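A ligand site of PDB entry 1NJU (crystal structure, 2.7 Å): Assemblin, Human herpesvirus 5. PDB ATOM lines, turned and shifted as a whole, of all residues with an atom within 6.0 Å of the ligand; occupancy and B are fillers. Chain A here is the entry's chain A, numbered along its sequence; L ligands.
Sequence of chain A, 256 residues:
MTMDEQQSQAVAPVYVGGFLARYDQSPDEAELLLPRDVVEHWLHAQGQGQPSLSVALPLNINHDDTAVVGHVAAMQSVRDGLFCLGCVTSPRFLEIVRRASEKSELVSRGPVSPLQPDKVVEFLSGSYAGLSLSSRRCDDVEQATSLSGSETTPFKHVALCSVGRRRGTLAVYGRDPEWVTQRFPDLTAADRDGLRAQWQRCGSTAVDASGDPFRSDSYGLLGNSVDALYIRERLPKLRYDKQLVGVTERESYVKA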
ATOM      1  N   GLU A  31      -7.448  37.159  20.153  1.00  0.00           N
ATOM      2  CA  GLU A  31      -7.759  35.747  20.406  1.00  0.00           C
ATOM      3  C   GLU A  31      -6.676  34.789  19.936  1.00  0.00           C
ATOM      4  O   GLU A  31      -6.730  33.593  20.224  1.00  0.00           O
ATOM      5  CB  GLU A  31      -9.095  35.358  19.778  1.00  0.00           C
ATOM      6  CG  GLU A  31      -9.134  35.415  18.252  1.00  0.00           C
ATOM      7  CD  GLU A  31     -10.420  34.814  17.686  1.00  0.00           C
ATOM      8  OE1 GLU A  31     -11.509  35.234  18.136  1.00  0.00           O
ATOM      9  OE2 GLU A  31     -10.349  33.936  16.804  1.00  0.00           O
ATOM     10  N   LEU A  32      -5.683  35.290  19.205  1.00  0.00           N
ATOM     11  CA  LEU A  32      -4.604  34.456  18.714  1.00  0.00           C
ATOM     12  C   LEU A  32      -3.406  34.451  19.654  1.00  0.00           C
ATOM     13  O   LEU A  32      -2.421  33.751  19.425  1.00  0.00           O
ATOM     14  CB  LEU A  32      -4.164  34.915  17.315  1.00  0.00           C
ATOM     15  CG  LEU A  32      -4.851  34.217  16.134  1.00  0.00           C
ATOM     16  CD1 LEU A  32      -6.216  33.705  16.530  1.00  0.00           C
ATOM     17  CD2 LEU A  32      -4.942  35.188  14.975  1.00  0.00           C
ATOM     18  N   ASN A  62      -7.360  21.887   6.897  1.00  0.00           N
ATOM     19  CA  ASN A  62      -8.112  23.107   7.189  1.00  0.00           C
ATOM     20  C   ASN A  62      -9.224  22.908   8.215  1.00  0.00           C
ATOM     21  O   ASN A  62     -10.385  23.241   7.975  1.00  0.00           O
ATOM     22  CB  ASN A  62      -8.676  23.685   5.881  1.00  0.00           C
ATOM     23  CG  ASN A  62      -9.424  25.004   6.077  1.00  0.00           C
ATOM     24  OD1 ASN A  62      -8.899  25.940   6.696  1.00  0.00           O
ATOM     25  ND2 ASN A  62     -10.641  25.086   5.536  1.00  0.00           N
ATOM     26  N   HIS A  63      -8.859  22.342   9.359  1.00  0.00           N
ATOM     27  CA  HIS A  63      -9.755  22.099  10.488  1.00  0.00           C
ATOM     28  C   HIS A  63     -10.979  21.209  10.290  1.00  0.00           C
ATOM     29  O   HIS A  63     -11.816  21.136  11.177  1.00  0.00           O
ATOM     30  CB  HIS A  63     -10.225  23.441  11.060  1.00  0.00           C
ATOM     31  CG  HIS A  63      -9.095  24.290  11.563  1.00  0.00           C
ATOM     32  ND1 HIS A  63      -8.385  23.981  12.693  1.00  0.00           N
ATOM     33  CD2 HIS A  63      -8.535  25.408  11.050  1.00  0.00           C
ATOM     34  CE1 HIS A  63      -7.420  24.872  12.860  1.00  0.00           C
ATOM     35  NE2 HIS A  63      -7.490  25.745  11.875  1.00  0.00           N
ATOM     36  N   LEU A 131       0.576  25.823   9.097  1.00  0.00           N
ATOM     37  CA  LEU A 131      -0.004  25.037  10.188  1.00  0.00           C
ATOM     38  C   LEU A 131      -0.929  25.963  10.952  1.00  0.00           C
ATOM     39  O   LEU A 131      -0.682  27.167  11.057  1.00  0.00           O
ATOM     40  CB  LEU A 131       1.069  24.501  11.149  1.00  0.00           C
ATOM     41  CG  LEU A 131       2.098  23.433  10.750  1.00  0.00           C
ATOM     42  CD1 LEU A 131       1.514  22.490   9.687  1.00  0.00           C
ATOM     43  CD2 LEU A 131       3.338  24.147  10.223  1.00  0.00           C
ATOM     44  N   SER A 132      -2.002  25.401  11.489  1.00  0.00           N
ATOM     45  CA  SER A 132      -2.950  26.194  12.251  1.00  0.00           C
ATOM     46  C   SER A 132      -3.433  25.375  13.406  1.00  0.00           C
ATOM     47  O   SER A 132      -4.085  24.349  13.228  1.00  0.00           O
ATOM     48  CB  SER A 132      -4.127  26.589  11.377  1.00  0.00           C
ATOM     49  OG  SER A 132      -5.114  27.239  12.163  1.00  0.00           O
ATOM     50  N   LEU A 133      -3.097  25.827  14.596  1.00  0.00           N
ATOM     51  CA  LEU A 133      -3.481  25.132  15.819  1.00  0.00           C
ATOM     52  C   LEU A 133      -4.952  25.318  16.129  1.00  0.00           C
ATOM     53  O   LEU A 133      -5.609  26.229  15.618  1.00  0.00           O
ATOM     54  CB  LEU A 133      -2.643  25.666  16.980  1.00  0.00           C
ATOM     55  CG  LEU A 133      -2.879  25.058  18.354  1.00  0.00           C
ATOM     56  CD1 LEU A 133      -2.510  23.583  18.319  1.00  0.00           C
ATOM     57  CD2 LEU A 133      -2.067  25.831  19.385  1.00  0.00           C
ATOM     58  N   SER A 134      -5.466  24.431  16.948  1.00  0.00           N
ATOM     59  CA  SER A 134      -6.845  24.504  17.390  1.00  0.00           C
ATOM     60  C   SER A 134      -6.704  24.341  18.900  1.00  0.00           C
ATOM     61  O   SER A 134      -6.438  23.256  19.397  1.00  0.00           O
ATOM     62  CB  SER A 134      -7.660  23.353  16.799  1.00  0.00           C
ATOM     63  OG  SER A 134      -9.000  23.415  17.235  1.00  0.00           O
ATOM     64  N   SER A 135      -6.842  25.445  19.614  1.00  0.00           N
ATOM     65  CA  SER A 135      -6.709  25.423  21.055  1.00  0.00           C
ATOM     66  C   SER A 135      -7.872  26.131  21.728  1.00  0.00           C
ATOM     67  O   SER A 135      -8.656  26.822  21.074  1.00  0.00           O
ATOM     68  CB  SER A 135      -5.369  26.050  21.454  1.00  0.00           C
ATOM     69  OG  SER A 135      -5.089  27.203  20.679  1.00  0.00           O
ATOM     70  N   ARG A 136      -7.981  25.947  23.042  1.00  0.00           N
ATOM     71  CA  ARG A 136      -9.050  26.569  23.815  1.00  0.00           C
ATOM     72  C   ARG A 136      -8.821  28.067  23.939  1.00  0.00           C
ATOM     73  O   ARG A 136      -7.687  28.524  24.012  1.00  0.00           O
ATOM     74  CB  ARG A 136      -9.143  25.910  25.196  1.00  0.00           C
ATOM     75  CG  ARG A 136      -8.241  26.462  26.283  1.00  0.00           C
ATOM     76  CD  ARG A 136      -8.486  25.727  27.620  1.00  0.00           C
ATOM     77  NE  ARG A 136      -9.860  25.211  27.717  1.00  0.00           N
ATOM     78  CZ  ARG A 136     -10.216  23.952  27.487  1.00  0.00           C
ATOM     79  NH1 ARG A 136      -9.307  23.043  27.138  1.00  0.00           N
ATOM     80  NH2 ARG A 136     -11.494  23.582  27.561  1.00  0.00           N
ATOM     81  N   ARG A 137      -9.911  28.835  23.945  1.00  0.00           N
ATOM     82  CA  ARG A 137      -9.797  30.283  24.059  1.00  0.00           C
ATOM     83  C   ARG A 137      -8.968  30.688  25.262  1.00  0.00           C
ATOM     84  O   ARG A 137      -9.254  30.299  26.389  1.00  0.00           O
ATOM     85  CB  ARG A 137     -11.185  30.926  24.161  1.00  0.00           C
ATOM     86  CG  ARG A 137     -11.901  31.056  22.839  1.00  0.00           C
ATOM     87  CD  ARG A 137     -13.132  31.939  22.946  1.00  0.00           C
ATOM     88  NE  ARG A 137     -13.908  31.903  21.709  1.00  0.00           N
ATOM     89  CZ  ARG A 137     -13.484  32.387  20.541  1.00  0.00           C
ATOM     90  NH1 ARG A 137     -12.278  32.948  20.451  1.00  0.00           N
ATOM     91  NH2 ARG A 137     -14.258  32.305  19.463  1.00  0.00           N
ATOM     92  N   CYS A 138      -7.930  31.477  25.014  1.00  0.00           N
ATOM     93  CA  CYS A 138      -7.061  31.943  26.083  1.00  0.00           C
ATOM     94  C   CYS A 138      -7.721  33.104  26.826  1.00  0.00           C
ATOM     95  O   CYS A 138      -8.168  32.948  27.967  1.00  0.00           O
ATOM     96  CB  CYS A 138      -5.717  32.379  25.506  1.00  0.00           C
ATOM     97  SG  CYS A 138      -4.634  33.193  26.687  1.00  0.00           S
ATOM     98  N   LYS A 156      -6.642  21.012  20.912  1.00  0.00           N
ATOM     99  CA  LYS A 156      -7.609  20.162  20.208  1.00  0.00           C
ATOM    100  C   LYS A 156      -6.974  19.366  19.057  1.00  0.00           C
ATOM    101  O   LYS A 156      -7.050  18.143  19.027  1.00  0.00           O
ATOM    102  CB  LYS A 156      -8.770  21.011  19.701  1.00  0.00           C
ATOM    103  CG  LYS A 156      -9.667  20.289  18.680  1.00  0.00           C
ATOM    104  CD  LYS A 156     -10.412  19.070  19.281  1.00  0.00           C
ATOM    105  CE  LYS A 156     -11.156  18.278  18.186  1.00  0.00           C
ATOM    106  NZ  LYS A 156     -10.222  17.574  17.228  1.00  0.00           N
ATOM    107  N   HIS A 157      -6.363  20.076  18.107  1.00  0.00           N
ATOM    108  CA  HIS A 157      -5.693  19.437  16.961  1.00  0.00           C
ATOM    109  C   HIS A 157      -4.865  20.431  16.166  1.00  0.00           C
ATOM    110  O   HIS A 157      -4.825  21.618  16.476  1.00  0.00           O
ATOM    111  CB  HIS A 157      -6.727  18.773  16.027  1.00  0.00           C
ATOM    112  CG  HIS A 157      -7.645  19.752  15.352  1.00  0.00           C
ATOM    113  ND1 HIS A 157      -8.962  19.929  15.737  1.00  0.00           N
ATOM    114  CD2 HIS A 157      -7.425  20.645  14.359  1.00  0.00           C
ATOM    115  CE1 HIS A 157      -9.502  20.882  15.001  1.00  0.00           C
ATOM    116  NE2 HIS A 157      -8.595  21.330  14.160  1.00  0.00           N
ATOM    117  N   CYS A 161      -2.920  23.831   6.302  1.00  0.00           N
ATOM    118  CA  CYS A 161      -3.715  24.812   5.567  1.00  0.00           C
ATOM    119  C   CYS A 161      -2.882  25.584   4.554  1.00  0.00           C
ATOM    120  O   CYS A 161      -1.651  25.510   4.563  1.00  0.00           O
ATOM    121  CB  CYS A 161      -4.327  25.769   6.560  1.00  0.00           C
ATOM    122  SG  CYS A 161      -3.099  26.339   7.753  1.00  0.00           S
ATOM    123  N   SER A 162      -3.558  26.343   3.698  1.00  0.00           N
ATOM    124  CA  SER A 162      -2.893  27.140   2.668  1.00  0.00           C
ATOM    125  C   SER A 162      -2.014  28.217   3.273  1.00  0.00           C
ATOM    126  O   SER A 162      -1.012  28.622   2.680  1.00  0.00           O
ATOM    127  CB  SER A 162      -3.923  27.802   1.745  1.00  0.00           C
ATOM    128  OG  SER A 162      -4.371  26.880   0.781  1.00  0.00           O
ATOM    129  N   VAL A 163      -2.392  28.701   4.455  1.00  0.00           N
ATOM    130  CA  VAL A 163      -1.625  29.711   5.148  1.00  0.00           C
ATOM    131  C   VAL A 163      -2.247  29.862   6.524  1.00  0.00           C
ATOM    132  O   VAL A 163      -3.462  29.787   6.663  1.00  0.00           O
ATOM    133  CB  VAL A 163      -1.671  31.038   4.388  1.00  0.00           C
ATOM    134  CG1 VAL A 163      -3.126  31.473   4.214  1.00  0.00           C
ATOM    135  CG2 VAL A 163      -0.831  32.101   5.118  1.00  0.00           C
ATOM    136  N   GLY A 164      -1.425  30.063   7.539  1.00  0.00           N
ATOM    137  CA  GLY A 164      -1.966  30.178   8.872  1.00  0.00           C
ATOM    138  C   GLY A 164      -2.274  31.577   9.357  1.00  0.00           C
ATOM    139  O   GLY A 164      -1.771  32.561   8.805  1.00  0.00           O
ATOM    140  N   ARG A 165      -3.092  31.666  10.391  1.00  0.00           N
ATOM    141  CA  ARG A 165      -3.450  32.940  10.981  1.00  0.00           C
ATOM    142  C   ARG A 165      -2.288  33.509  11.780  1.00  0.00           C
ATOM    143  O   ARG A 165      -2.134  34.727  11.898  1.00  0.00           O
ATOM    144  CB  ARG A 165      -4.674  32.770  11.864  1.00  0.00           C
ATOM    145  CG  ARG A 165      -5.931  32.389  11.111  1.00  0.00           C
ATOM    146  CD  ARG A 165      -7.060  33.351  11.430  1.00  0.00           C
ATOM    147  NE  ARG A 165      -7.701  33.053  12.704  1.00  0.00           N
ATOM    148  CZ  ARG A 165      -8.119  33.978  13.557  1.00  0.00           C
ATOM    149  NH1 ARG A 165      -7.977  35.257  13.269  1.00  0.00           N
ATOM    150  NH2 ARG A 165      -8.715  33.620  14.691  1.00  0.00           N
ATOM    151  N   ARG A 166      -1.472  32.619  12.356  1.00  0.00           N
ATOM    152  CA  ARG A 166      -0.324  33.028  13.143  1.00  0.00           C
ATOM    153  C   ARG A 166       0.912  33.001  12.252  1.00  0.00           C
ATOM    154  O   ARG A 166       1.199  31.988  11.598  1.00  0.00           O
ATOM    155  CB  ARG A 166      -0.107  32.083  14.338  1.00  0.00           C
ATOM    156  CG  ARG A 166      -1.304  31.943  15.254  1.00  0.00           C
ATOM    157  CD  ARG A 166      -0.847  31.632  16.660  1.00  0.00           C
ATOM    158  NE  ARG A 166      -1.932  31.577  17.639  1.00  0.00           N
ATOM    159  CZ  ARG A 166      -2.806  30.587  17.749  1.00  0.00           C
ATOM    160  NH1 ARG A 166      -2.744  29.535  16.939  1.00  0.00           N
ATOM    161  NH2 ARG A 166      -3.750  30.635  18.681  1.00  0.00           N
ATOM    162  N   THR A 169       4.021  30.125  11.088  1.00  0.00           N
ATOM    163  CA  THR A 169       3.423  28.802  11.069  1.00  0.00           C
ATOM    164  C   THR A 169       3.611  28.039   9.770  1.00  0.00           C
ATOM    165  O   THR A 169       2.811  27.148   9.453  1.00  0.00           O
ATOM    166  CB  THR A 169       1.938  28.894  11.360  1.00  0.00           C
ATOM    167  OG1 THR A 169       1.330  29.770  10.385  1.00  0.00           O
ATOM    168  CG2 THR A 169       1.706  29.457  12.763  1.00  0.00           C
ATOM    169  N   ILE A 231      -8.010  33.866   0.321  1.00  0.00           N
ATOM    170  CA  ILE A 231      -7.401  34.324   1.558  1.00  0.00           C
ATOM    171  C   ILE A 231      -6.571  35.526   1.114  1.00  0.00           C
ATOM    172  O   ILE A 231      -5.963  35.511   0.031  1.00  0.00           O
ATOM    173  CB  ILE A 231      -6.468  33.265   2.168  1.00  0.00           C
ATOM    174  CG1 ILE A 231      -7.217  31.946   2.344  1.00  0.00           C
ATOM    175  CG2 ILE A 231      -5.984  33.757   3.517  1.00  0.00           C
ATOM    176  CD1 ILE A 231      -6.441  30.882   3.119  1.00  0.00           C
ATOM    177  N   LYS A 237       2.297  36.529   3.045  1.00  0.00           N
ATOM    178  CA  LYS A 237       2.427  36.021   4.416  1.00  0.00           C
ATOM    179  C   LYS A 237       3.371  34.833   4.463  1.00  0.00           C
ATOM    180  O   LYS A 237       4.284  34.781   5.288  1.00  0.00           O
ATOM    181  CB  LYS A 237       1.068  35.600   5.001  1.00  0.00           C
ATOM    182  CG  LYS A 237       0.184  36.777   5.411  1.00  0.00           C
ATOM    183  CD  LYS A 237      -1.170  36.283   5.866  1.00  0.00           C
ATOM    184  CE  LYS A 237      -2.168  37.421   6.039  1.00  0.00           C
ATOM    185  NZ  LYS A 237      -3.540  36.876   6.346  1.00  0.00           N
HETATM  186  C1  LIG L   1     -14.414  27.999  23.505  1.00  0.00           C
HETATM  187  C2  LIG L   1     -13.138  27.582  22.792  1.00  0.00           C
HETATM  188  O1  LIG L   1     -12.107  27.351  23.430  1.00  0.00           O
HETATM  189  C3  LIG L   1     -14.978  29.315  22.959  1.00  0.00           C
HETATM  190  C4  LIG L   1     -16.100  29.850  23.863  1.00  0.00           C
HETATM  191  C5  LIG L   1     -16.905  28.689  24.447  1.00  0.00           C
HETATM  192  C6  LIG L   1     -17.867  29.132  25.546  1.00  0.00           C
HETATM  193  N1  LIG L   1     -18.604  27.952  26.116  1.00  0.00           N
HETATM  194  N2  LIG L   1     -13.204  27.466  21.472  1.00  0.00           N
HETATM  195  C7  LIG L   1     -12.032  27.047  20.698  1.00  0.00           C
HETATM  196  C8  LIG L   1     -12.294  25.661  20.037  1.00  0.00           C
HETATM  197  C9  LIG L   1     -13.599  25.690  19.273  1.00  0.00           C
HETATM  198  C10 LIG L   1     -11.148  25.330  19.072  1.00  0.00           C
HETATM  199  C11 LIG L   1     -12.373  24.581  21.106  1.00  0.00           C
HETATM  200  C12 LIG L   1     -11.644  28.071  19.641  1.00  0.00           C
HETATM  201  O2  LIG L   1     -12.498  28.690  19.011  1.00  0.00           O
HETATM  202  N3  LIG L   1     -10.337  28.242  19.438  1.00  0.00           N
HETATM  203  C13 LIG L   1      -9.833  29.182  18.447  1.00  0.00           C
HETATM  204  C14 LIG L   1      -8.973  30.287  19.090  1.00  0.00           C
HETATM  205  C15 LIG L   1      -7.715  29.690  19.666  1.00  0.00           C
HETATM  206  C16 LIG L   1      -8.626  31.320  18.054  1.00  0.00           C
HETATM  207  C17 LIG L   1      -9.759  30.943  20.191  1.00  0.00           C
HETATM  208  C18 LIG L   1      -8.974  28.447  17.410  1.00  0.00           C
HETATM  209  O3  LIG L   1      -8.010  27.768  17.759  1.00  0.00           O
HETATM  210  N4  LIG L   1      -9.341  28.597  16.146  1.00  0.00           N
HETATM  211  C19 LIG L   1      -8.619  27.947  15.065  1.00  0.00           C
HETATM  212  C20 LIG L   1      -9.598  27.168  14.177  1.00  0.00           C
HETATM  213  C21 LIG L   1     -10.305  26.061  14.928  1.00  0.00           C
HETATM  214  O4  LIG L   1      -9.892  25.699  16.041  1.00  0.00           O
HETATM  215  N5  LIG L   1     -11.371  25.496  14.332  1.00  0.00           N
HETATM  216  C22 LIG L   1     -11.889  25.856  13.044  1.00  0.00           C
HETATM  217  C23 LIG L   1     -12.080  24.453  14.976  1.00  0.00           C
HETATM  218  C24 LIG L   1      -7.835  28.925  14.195  1.00  0.00           C
HETATM  219  O5  LIG L   1      -8.349  29.980  13.800  1.00  0.00           O
HETATM  220  N6  LIG L   1      -6.585  28.570  13.908  1.00  0.00           N
HETATM  221  C25 LIG L   1      -5.723  29.392  13.066  1.00  0.00           C
HETATM  222  C26 LIG L   1      -5.298  28.608  11.795  1.00  0.00           C
HETATM  223  O6  LIG L   1      -4.110  29.173  11.327  1.00  0.00           O
HETATM  224  C27 LIG L   1      -4.484  29.803  13.857  1.00  0.00           C
HETATM  225  C28 LIG L   1      -6.406  28.685  10.694  1.00  0.00           C
HETATM  226  O7  LIG L   1      -7.593  28.419  10.955  1.00  0.00           O
HETATM  227  N7  LIG L   1      -6.015  29.042   9.461  1.00  0.00           N
HETATM  228  C29 LIG L   1      -6.918  29.173   8.310  1.00  0.00           C
HETATM  229  C30 LIG L   1      -6.377  28.395   7.079  1.00  0.00           C
HETATM  230  C31 LIG L   1      -6.971  28.916   5.771  1.00  0.00           C
HETATM  231  C32 LIG L   1      -7.072  30.625   7.924  1.00  0.00           C
HETATM  232  C33 LIG L   1      -8.320  31.236   7.970  1.00  0.00           C
HETATM  233  C34 LIG L   1      -8.478  32.568   7.605  1.00  0.00           C
HETATM  234  C35 LIG L   1      -7.379  33.309   7.175  1.00  0.00           C
HETATM  235  C36 LIG L   1      -6.136  32.711   7.109  1.00  0.00           C
HETATM  236  C37 LIG L   1      -5.990  31.375   7.495  1.00  0.00           C
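A carbon (C26) of the ligand is bonded to the side-chain hydroxyl of Ser 132. The backbone NH of Arg 137 lies within hydrogen-bond range of an oxygen (O1) of the ligand, 2.7 Å away. The side-chain hydroxyl (OG) of Ser 134 is in hydrogen-bond range of an oxygen (O4) of the ligand (2.7 Å). The backbone NH (N) of Ser 135 is in hydrogen-bond range of an oxygen (O3) of the ligand (3.2 Å). The backbone carbonyl oxygen (O) of Ser 135 lies within hydrogen-bond range of a nitrogen (N3) of the ligand, at 2.7 Å. NE2 of His 63 is in hydrogen-bond range of O7 of the ligand (2.8 Å). O6 of the ligand sits at hydrogen-bond distance from N of Arg 165, 2.9 Å away. An oxygen (O5) of the ligand is in hydrogen-bond range of the guanidinium group of Arg 165 (3.3 Å). A nitrogen (N6) of the ligand sits at hydrogen-bond distance from the backbone carbonyl oxygen (O) of Leu 133, 3.1 Å away.
The side-chain hydroxyl of Ser 132 lies within hydrogen-bond range of a ring nitrogen (NE2) of His 63 (2.8 Å). NH1 of Arg 137 is in salt-bridge range of OE1 of Glu 31. The backbone carbonyl oxygen of His 157 is in hydrogen-bond range of the backbone NH of Ser 134, 2.9 Å away. The backbone NH (N) of Lys 156 lies within hydrogen-bond range of the backbone carbonyl oxygen (O) of Ser 134 (2.7 Å). A ring nitrogen (NE2) of His 157 sits at hydrogen-bond distance from a ring nitrogen (ND1) of His 63 (3.0 Å). O of Leu 32 sits at hydrogen-bond distance from NE of Arg 166, at 2.9 Å. The backbone carbonyl oxygen (O) of Arg 166 lies within hydrogen-bond range of the side-chain hydroxyl (OG1) of Thr 169 (2.5 Å). N of Leu 131 is in hydrogen-bond range of O of Thr 169.
Residues that only touch the ligand: Val 163 (3.1 Å), Arg 136 (3.2 Å), Ile 231 (3.3 Å), Cys 161 (3.4 Å), Glu 31 (3.4 Å), Gly 164 (3.4 Å), Asn 62 (3.5 Å), Arg 166 (3.5 Å), Leu 32 (3.7 Å) and Leu 131 (3.98 Å). Hydrophobic or aromatic side chains that line the ligand: Leu 32, His 63 and Ile 231. Within 4 Å of the ligand: Glu 31, Leu 32, Asn 62, His 63, Leu 131, Ser 132, Leu 133, Ser 134, Ser 135, Arg 136, Arg 137, Cys 161, Val 163, Gly 164, Arg 165, Arg 166 and Ile 231.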
